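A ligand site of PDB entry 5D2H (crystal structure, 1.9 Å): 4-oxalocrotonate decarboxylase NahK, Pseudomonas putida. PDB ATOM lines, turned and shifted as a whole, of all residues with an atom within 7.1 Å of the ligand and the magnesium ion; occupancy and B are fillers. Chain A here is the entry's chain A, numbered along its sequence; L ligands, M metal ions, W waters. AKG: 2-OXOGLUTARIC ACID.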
ATOM      1  N   LYS A  83      -0.961  -4.982  27.739  1.00  0.00           N
ATOM      2  CA  LYS A  83      -0.371  -4.560  26.487  1.00  0.00           C
ATOM      3  C   LYS A  83       0.267  -3.211  26.687  1.00  0.00           C
ATOM      4  O   LYS A  83      -0.090  -2.501  27.636  1.00  0.00           O
ATOM      5  CB  LYS A  83      -1.389  -4.563  25.339  1.00  0.00           C
ATOM      6  CG  LYS A  83      -2.678  -3.784  25.574  1.00  0.00           C
ATOM      7  CD  LYS A  83      -2.451  -2.288  25.525  1.00  0.00           C
ATOM      8  CE  LYS A  83      -2.007  -1.834  24.140  1.00  0.00           C
ATOM      9  NZ  LYS A  83      -3.121  -1.827  23.142  1.00  0.00           N
ATOM     10  N   MET A  84       1.237  -2.877  25.852  1.00  0.00           N
ATOM     11  CA  MET A  84       1.963  -1.622  25.992  1.00  0.00           C
ATOM     12  C   MET A  84       1.674  -0.738  24.804  1.00  0.00           C
ATOM     13  O   MET A  84       1.653  -1.212  23.673  1.00  0.00           O
ATOM     14  CB  MET A  84       3.468  -1.854  26.067  1.00  0.00           C
ATOM     15  CG  MET A  84       3.897  -2.739  27.190  1.00  0.00           C
ATOM     16  SD  MET A  84       3.366  -2.000  28.719  1.00  0.00           S
ATOM     17  CE  MET A  84       4.434  -0.570  28.840  1.00  0.00           C
ATOM     18  N   GLY A  85       1.459   0.545  25.073  1.00  0.00           N
ATOM     19  CA  GLY A  85       1.300   1.524  24.014  1.00  0.00           C
ATOM     20  C   GLY A  85       2.368   2.593  24.099  1.00  0.00           C
ATOM     21  O   GLY A  85       2.988   2.778  25.159  1.00  0.00           O
ATOM     22  N   LEU A  86       2.581   3.313  22.999  1.00  0.00           N
ATOM     23  CA  LEU A  86       3.544   4.411  22.980  1.00  0.00           C
ATOM     24  C   LEU A  86       4.941   3.898  23.347  1.00  0.00           C
ATOM     25  O   LEU A  86       5.615   4.466  24.200  1.00  0.00           O
ATOM     26  CB  LEU A  86       3.120   5.503  23.964  1.00  0.00           C
ATOM     27  CG  LEU A  86       1.858   6.264  23.553  1.00  0.00           C
ATOM     28  CD1 LEU A  86       1.587   7.377  24.546  1.00  0.00           C
ATOM     29  CD2 LEU A  86       2.033   6.811  22.150  1.00  0.00           C
ATOM     30  N   THR A  87       5.338   2.804  22.712  1.00  0.00           N
ATOM     31  CA  THR A  87       6.625   2.184  22.998  1.00  0.00           C
ATOM     32  C   THR A  87       7.635   2.668  21.982  1.00  0.00           C
ATOM     33  O   THR A  87       8.477   1.918  21.512  1.00  0.00           O
ATOM     34  CB  THR A  87       6.549   0.649  22.881  1.00  0.00           C
ATOM     35  OG1 THR A  87       5.969   0.300  21.626  1.00  0.00           O
ATOM     36  CG2 THR A  87       5.722   0.066  24.024  1.00  0.00           C
ATOM     37  N   SER A  88       7.516   3.945  21.625  1.00  0.00           N
ATOM     38  CA  SER A  88       8.427   4.559  20.687  1.00  0.00           C
ATOM     39  C   SER A  88       8.897   5.875  21.268  1.00  0.00           C
ATOM     40  O   SER A  88       8.077   6.725  21.638  1.00  0.00           O
ATOM     41  CB  SER A  88       7.721   4.821  19.356  1.00  0.00           C
ATOM     42  OG  SER A  88       8.398   5.814  18.613  1.00  0.00           O
ATOM     43  N   LYS A  91       7.531   8.653  19.314  1.00  0.00           N
ATOM     44  CA  LYS A  91       6.105   8.880  19.485  1.00  0.00           C
ATOM     45  C   LYS A  91       5.820   9.497  20.851  1.00  0.00           C
ATOM     46  O   LYS A  91       4.962  10.366  20.981  1.00  0.00           O
ATOM     47  CB  LYS A  91       5.294   7.591  19.280  1.00  0.00           C
ATOM     48  CG  LYS A  91       3.850   7.840  18.855  1.00  0.00           C
ATOM     49  CD  LYS A  91       3.001   6.566  18.915  1.00  0.00           C
ATOM     50  CE  LYS A  91       1.581   6.800  18.351  1.00  0.00           C
ATOM     51  NZ  LYS A  91       1.500   6.626  16.856  1.00  0.00           N
ATOM     52  N   MET A  95       3.919  12.927  21.410  1.00  0.00           N
ATOM     53  CA  MET A  95       2.700  13.033  22.214  1.00  0.00           C
ATOM     54  C   MET A  95       2.923  13.774  23.533  1.00  0.00           C
ATOM     55  O   MET A  95       1.989  13.952  24.313  1.00  0.00           O
ATOM     56  CB  MET A  95       2.100  11.661  22.492  1.00  0.00           C
ATOM     57  CG  MET A  95       1.777  10.880  21.248  1.00  0.00           C
ATOM     58  SD  MET A  95       0.842  11.886  20.074  1.00  0.00           S
ATOM     59  CE  MET A  95       0.846  10.821  18.646  1.00  0.00           C
ATOM     60  N   ILE A 101       2.448   3.714  27.713  1.00  0.00           N
ATOM     61  CA  ILE A 101       1.230   3.523  28.449  1.00  0.00           C
ATOM     62  C   ILE A 101       0.931   2.040  28.360  1.00  0.00           C
ATOM     63  O   ILE A 101       1.544   1.332  27.557  1.00  0.00           O
ATOM     64  CB  ILE A 101       0.057   4.292  27.827  1.00  0.00           C
ATOM     65  CG1 ILE A 101      -0.129   3.865  26.374  1.00  0.00           C
ATOM     66  CG2 ILE A 101       0.303   5.798  27.915  1.00  0.00           C
ATOM     67  CD1 ILE A 101      -1.412   4.391  25.760  1.00  0.00           C
ATOM     68  N   GLU A 128      -1.414  -4.444  14.549  1.00  0.00           N
ATOM     69  CA  GLU A 128       0.001  -4.189  14.685  1.00  0.00           C
ATOM     70  C   GLU A 128       0.724  -5.488  15.030  1.00  0.00           C
ATOM     71  O   GLU A 128       0.158  -6.366  15.700  1.00  0.00           O
ATOM     72  CB  GLU A 128       0.266  -3.098  15.732  1.00  0.00           C
ATOM     73  CG  GLU A 128      -0.555  -3.225  16.979  1.00  0.00           C
ATOM     74  CD  GLU A 128      -0.396  -2.036  17.907  1.00  0.00           C
ATOM     75  OE1 GLU A 128       0.257  -1.032  17.540  1.00  0.00           O
ATOM     76  OE2 GLU A 128      -0.933  -2.101  19.031  1.00  0.00           O
ATOM     77  N   ALA A 129       1.948  -5.610  14.540  1.00  0.00           N
ATOM     78  CA  ALA A 129       2.806  -6.758  14.810  1.00  0.00           C
ATOM     79  C   ALA A 129       3.599  -6.519  16.077  1.00  0.00           C
ATOM     80  O   ALA A 129       4.262  -5.485  16.211  1.00  0.00           O
ATOM     81  CB  ALA A 129       3.745  -7.013  13.647  1.00  0.00           C
ATOM     82  N   GLU A 130       3.527  -7.468  17.000  1.00  0.00           N
ATOM     83  CA  GLU A 130       4.196  -7.314  18.274  1.00  0.00           C
ATOM     84  C   GLU A 130       4.845  -8.617  18.661  1.00  0.00           C
ATOM     85  O   GLU A 130       4.570  -9.684  18.091  1.00  0.00           O
ATOM     86  CB  GLU A 130       3.201  -6.871  19.356  1.00  0.00           C
ATOM     87  CG  GLU A 130       2.308  -5.718  18.954  1.00  0.00           C
ATOM     88  CD  GLU A 130       1.670  -4.988  20.135  1.00  0.00           C
ATOM     89  OE1 GLU A 130       0.661  -4.284  19.919  1.00  0.00           O
ATOM     90  OE2 GLU A 130       2.165  -5.084  21.280  1.00  0.00           O
ATOM     91  N   GLU A 161      -1.724  -7.477  17.486  1.00  0.00           N
ATOM     92  CA  GLU A 161      -2.801  -6.852  18.232  1.00  0.00           C
ATOM     93  C   GLU A 161      -3.768  -6.235  17.258  1.00  0.00           C
ATOM     94  O   GLU A 161      -3.374  -5.719  16.213  1.00  0.00           O
ATOM     95  CB  GLU A 161      -2.291  -5.800  19.218  1.00  0.00           C
ATOM     96  CG  GLU A 161      -3.392  -5.369  20.190  1.00  0.00           C
ATOM     97  CD  GLU A 161      -2.977  -4.325  21.224  1.00  0.00           C
ATOM     98  OE1 GLU A 161      -1.916  -3.694  21.083  1.00  0.00           O
ATOM     99  OE2 GLU A 161      -3.751  -4.140  22.188  1.00  0.00           O
ATOM    100  N   VAL A 162      -5.053  -6.330  17.571  1.00  0.00           N
ATOM    101  CA  VAL A 162      -6.029  -5.504  16.896  1.00  0.00           C
ATOM    102  C   VAL A 162      -6.389  -4.411  17.874  1.00  0.00           C
ATOM    103  O   VAL A 162      -6.891  -4.674  18.971  1.00  0.00           O
ATOM    104  CB  VAL A 162      -7.276  -6.300  16.444  1.00  0.00           C
ATOM    105  CG1 VAL A 162      -8.203  -5.408  15.620  1.00  0.00           C
ATOM    106  CG2 VAL A 162      -6.844  -7.516  15.613  1.00  0.00           C
ATOM    107  N   ILE A 163      -6.066  -3.178  17.502  1.00  0.00           N
ATOM    108  CA  ILE A 163      -6.400  -2.059  18.347  1.00  0.00           C
ATOM    109  C   ILE A 163      -7.545  -1.319  17.694  1.00  0.00           C
ATOM    110  O   ILE A 163      -7.718  -1.358  16.495  1.00  0.00           O
ATOM    111  CB  ILE A 163      -5.201  -1.123  18.577  1.00  0.00           C
ATOM    112  CG1 ILE A 163      -4.668  -0.604  17.230  1.00  0.00           C
ATOM    113  CG2 ILE A 163      -4.120  -1.840  19.423  1.00  0.00           C
ATOM    114  CD1 ILE A 163      -3.553   0.411  17.372  1.00  0.00           C
ATOM    115  N   ASP A 164      -8.351  -0.668  18.519  1.00  0.00           N
ATOM    116  CA  ASP A 164      -9.554  -0.048  18.011  1.00  0.00           C
ATOM    117  C   ASP A 164      -9.931   0.999  19.026  1.00  0.00           C
ATOM    118  O   ASP A 164     -10.567   0.712  20.038  1.00  0.00           O
ATOM    119  CB  ASP A 164     -10.656  -1.102  17.864  1.00  0.00           C
ATOM    120  CG  ASP A 164     -11.880  -0.588  17.120  1.00  0.00           C
ATOM    121  OD1 ASP A 164     -11.729   0.323  16.282  1.00  0.00           O
ATOM    122  OD2 ASP A 164     -12.993  -1.095  17.375  1.00  0.00           O
ATOM    123  N   SER A 165      -9.493   2.229  18.781  1.00  0.00           N
ATOM    124  CA  SER A 165      -9.818   3.319  19.655  1.00  0.00           C
ATOM    125  C   SER A 165     -11.332   3.494  19.621  1.00  0.00           C
ATOM    126  O   SER A 165     -11.921   3.513  18.538  1.00  0.00           O
ATOM    127  CB  SER A 165      -9.152   4.603  19.186  1.00  0.00           C
ATOM    128  OG  SER A 165      -9.515   5.664  20.034  1.00  0.00           O
ATOM    129  N   PHE A 172      -4.413  11.571  18.071  1.00  0.00           N
ATOM    130  CA  PHE A 172      -4.106  10.733  19.223  1.00  0.00           C
ATOM    131  C   PHE A 172      -4.005  11.548  20.519  1.00  0.00           C
ATOM    132  O   PHE A 172      -3.293  12.559  20.586  1.00  0.00           O
ATOM    133  CB  PHE A 172      -2.781  10.005  18.975  1.00  0.00           C
ATOM    134  CG  PHE A 172      -2.438   8.995  20.019  1.00  0.00           C
ATOM    135  CD1 PHE A 172      -2.842   7.682  19.880  1.00  0.00           C
ATOM    136  CD2 PHE A 172      -1.693   9.351  21.130  1.00  0.00           C
ATOM    137  CE1 PHE A 172      -2.529   6.728  20.837  1.00  0.00           C
ATOM    138  CE2 PHE A 172      -1.377   8.414  22.100  1.00  0.00           C
ATOM    139  CZ  PHE A 172      -1.786   7.094  21.951  1.00  0.00           C
ATOM    140  N   VAL A 177      -6.660   7.843  25.475  1.00  0.00           N
ATOM    141  CA  VAL A 177      -6.340   6.483  25.035  1.00  0.00           C
ATOM    142  C   VAL A 177      -6.172   5.581  26.252  1.00  0.00           C
ATOM    143  O   VAL A 177      -6.690   4.465  26.273  1.00  0.00           O
ATOM    144  CB  VAL A 177      -5.124   6.464  24.095  1.00  0.00           C
ATOM    145  CG1 VAL A 177      -4.610   5.041  23.905  1.00  0.00           C
ATOM    146  CG2 VAL A 177      -5.497   7.081  22.743  1.00  0.00           C
ATOM    147  N   ASN A 181      -8.427   2.098  27.709  1.00  0.00           N
ATOM    148  CA  ASN A 181      -7.665   0.840  27.785  1.00  0.00           C
ATOM    149  C   ASN A 181      -6.638   0.714  26.658  1.00  0.00           C
ATOM    150  O   ASN A 181      -6.461  -0.368  26.083  1.00  0.00           O
ATOM    151  CB  ASN A 181      -8.597  -0.374  27.781  1.00  0.00           C
ATOM    152  CG  ASN A 181      -7.898  -1.644  28.224  1.00  0.00           C
ATOM    153  OD1 ASN A 181      -6.942  -1.609  29.017  1.00  0.00           O
ATOM    154  ND2 ASN A 181      -8.361  -2.784  27.724  1.00  0.00           N
ATOM    155  N   ALA A 182      -5.972   1.822  26.340  1.00  0.00           N
ATOM    156  CA  ALA A 182      -4.951   1.802  25.308  1.00  0.00           C
ATOM    157  C   ALA A 182      -5.508   1.194  24.013  1.00  0.00           C
ATOM    158  O   ALA A 182      -4.790   0.525  23.269  1.00  0.00           O
ATOM    159  CB  ALA A 182      -3.727   1.022  25.794  1.00  0.00           C
ATOM    160  N   SER A 183      -6.801   1.406  23.772  1.00  0.00           N
ATOM    161  CA  SER A 183      -7.421   0.992  22.502  1.00  0.00           C
ATOM    162  C   SER A 183      -7.430  -0.521  22.281  1.00  0.00           C
ATOM    163  O   SER A 183      -7.591  -1.008  21.159  1.00  0.00           O
ATOM    164  CB  SER A 183      -6.713   1.674  21.323  1.00  0.00           C
ATOM    165  OG  SER A 183      -6.597   3.075  21.546  1.00  0.00           O
ATOM    166  N   SER A 184      -7.256  -1.288  23.350  1.00  0.00           N
ATOM    167  CA  SER A 184      -7.168  -2.742  23.187  1.00  0.00           C
ATOM    168  C   SER A 184      -8.520  -3.271  22.716  1.00  0.00           C
ATOM    169  O   SER A 184      -9.560  -2.676  23.014  1.00  0.00           O
ATOM    170  CB  SER A 184      -6.771  -3.414  24.491  1.00  0.00           C
ATOM    171  OG  SER A 184      -5.648  -2.761  25.065  1.00  0.00           O
ATOM    172  N   MET A 252       2.081  -7.969  25.863  1.00  0.00           N
ATOM    173  CA  MET A 252       2.357  -7.546  24.495  1.00  0.00           C
ATOM    174  C   MET A 252       3.240  -6.300  24.538  1.00  0.00           C
ATOM    175  O   MET A 252       2.824  -5.272  25.040  1.00  0.00           O
ATOM    176  CB  MET A 252       1.049  -7.271  23.760  1.00  0.00           C
ATOM    177  CG  MET A 252       0.088  -8.460  23.831  1.00  0.00           C
ATOM    178  SD  MET A 252      -1.383  -8.224  22.814  1.00  0.00           S
ATOM    179  CE  MET A 252      -0.568  -7.812  21.272  1.00  0.00           C
ATOM    180  N   THR A 253       4.463  -6.404  24.025  1.00  0.00           N
ATOM    181  CA  THR A 253       5.498  -5.400  24.326  1.00  0.00           C
ATOM    182  C   THR A 253       5.444  -4.125  23.485  1.00  0.00           C
ATOM    183  O   THR A 253       6.102  -3.147  23.824  1.00  0.00           O
ATOM    184  CB  THR A 253       6.932  -6.001  24.263  1.00  0.00           C
ATOM    185  OG1 THR A 253       7.203  -6.488  22.947  1.00  0.00           O
ATOM    186  CG2 THR A 253       7.092  -7.127  25.281  1.00  0.00           C
ATOM    187  N   GLY A 254       4.672  -4.125  22.409  1.00  0.00           N
ATOM    188  CA  GLY A 254       4.465  -2.921  21.647  1.00  0.00           C
ATOM    189  C   GLY A 254       4.506  -3.091  20.133  1.00  0.00           C
ATOM    190  O   GLY A 254       5.044  -4.065  19.621  1.00  0.00           O
ATOM    191  N   GLY A 255       3.919  -2.122  19.429  1.00  0.00           N
ATOM    192  CA  GLY A 255       3.861  -2.168  17.977  1.00  0.00           C
ATOM    193  C   GLY A 255       5.239  -2.098  17.359  1.00  0.00           C
ATOM    194  O   GLY A 255       5.962  -1.116  17.552  1.00  0.00           O
ATOM    195  N   ALA A 259       0.686   0.782  12.657  1.00  0.00           N
ATOM    196  CA  ALA A 259      -0.596   0.093  12.678  1.00  0.00           C
ATOM    197  C   ALA A 259      -1.267   0.212  11.315  1.00  0.00           C
ATOM    198  O   ALA A 259      -1.146   1.226  10.637  1.00  0.00           O
ATOM    199  CB  ALA A 259      -1.498   0.640  13.774  1.00  0.00           C
HETATM  200  C1  AKG L   1      -0.951   0.484  21.166  1.00  0.00           C
HETATM  201  O1  AKG L   1       0.160   0.780  20.678  1.00  0.00           O
HETATM  202  O2  AKG L   1      -1.207  -0.707  21.508  1.00  0.00           O
HETATM  203  C2  AKG L   1      -1.989   1.511  21.315  1.00  0.00           C
HETATM  204  O5  AKG L   1      -3.148   1.182  21.100  1.00  0.00           O
HETATM  205  C3  AKG L   1      -1.768   2.952  21.724  1.00  0.00           C
HETATM  206  C4  AKG L   1      -0.324   3.419  21.744  1.00  0.00           C
HETATM  207  C5  AKG L   1       0.252   3.730  20.374  1.00  0.00           C
HETATM  208  O3  AKG L   1       1.479   3.532  20.247  1.00  0.00           O
HETATM  209  O4  AKG L   1      -0.484   4.156  19.438  1.00  0.00           O
HETATM  210 MG    MG M   1      -0.238  -2.696  20.693  1.00  0.00          MG
HETATM  211  O   HOH W   1       0.623  -3.286  22.418  1.00  0.00           O
HETATM  212  O   HOH W   2      -2.740   4.065  18.278  1.00  0.00           O
HETATM  213  O   HOH W   3       0.058   1.576  17.499  1.00  0.00           O
HETATM  214  O   HOH W   4       3.467   0.357  21.165  1.00  0.00           O
HETATM  215  O   HOH W   5       1.354  -1.381  20.301  1.00  0.00           O
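The backbone NH (N) of Leu 86 lies within hydrogen-bond range of an oxygen (O3) of the ligand (3.0 Å). NZ of Lys 83 lies close to O2 of the ligand, 2.8 Å away.
N of Met 84 sits at hydrogen-bond distance from O of Met 252, 3.0 Å away. The side-chain amino group of Lys 83 lies close to the side-chain hydroxyl of Ser 184, 3.3 Å away. The side-chain amino group (NZ) of Lys 83 is in hydrogen-bond range of the backbone carbonyl oxygen (O) of Ala 182, at 2.9 Å. The side-chain carboxylate (OE2) of Glu 130 is in hydrogen-bond range of the backbone NH (N) of Gly 254. O of Ser 183 lies within hydrogen-bond range of N of Asp 164 (2.8 Å). The backbone carbonyl oxygen (O) of Ile 101 is in hydrogen-bond range of the backbone NH (N) of Gly 85, at 2.6 Å. The backbone NH (N) of Ala 182 lies within hydrogen-bond range of the backbone carbonyl oxygen (O) of Val 177 (2.7 Å). NZ of Lys 83 is in salt-bridge range of OE2 of Glu 161.
The backbone carbonyl oxygen of Ala 182 lies close to an oxygen (O5) of the ligand. Merely in contact with the ligand: Met 84 (3.6 Å), Gly 85 (3.4 Å), Lys 91 (3.5 Å), Ile 163 (3.6 Å), Phe 172 (3.6 Å) and Ser 183 (3.6 Å). Hydrophobic or aromatic side chains within 4 Å of the ligand: Leu 86, Ile 163 and Phe 172. Of the 28 residues printed, 11 come within 4 Å of the ligand. The nearest printed residue that does not touch the ligand is Val 177 (4.1 Å).
Lys 83 touches the magnesium ion (NZ to MG, 3.9 Å). Met 84 touches the magnesium ion (O to MG, 3.8 Å). Within 4 Å of the magnesium ion: Lys 83, Met 84, Glu 128, Glu 130 and Glu 161. Along chain A the residues within 4 Å of the magnesium ion span positions 83 to 161.
The magnesium ion is bound by OE2 of Glu 128 (1.9 Å), OE1 of Glu 130 (2.0 Å), OE1 of Glu 161 (2.0 Å), water W1 (2.0 Å), water W5 (2.1 Å) and O2 of the ligand (2.4 Å).
Water W1 lies within hydrogen-bond range of OE2 of Glu 130 (2.6 Å) and O of Met 84 (2.6 Å). Water W5 lies within hydrogen-bond range of an oxygen (O1) of the ligand, the backbone NH of Gly 255, the side-chain carboxylate of Glu 128 and the backbone carbonyl oxygen of Met 84. Water W3 bridges the side-chain carboxylate of Glu 128 and an oxygen (O4) of the ligand. Water W4 lies within hydrogen-bond range of the side-chain hydroxyl of Thr 87 (2.5 Å), the backbone NH of Gly 255 (3.1 Å), an oxygen (O1) of the ligand (3.4 Å) and the backbone carbonyl oxygen of Met 84 (3.5 Å).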
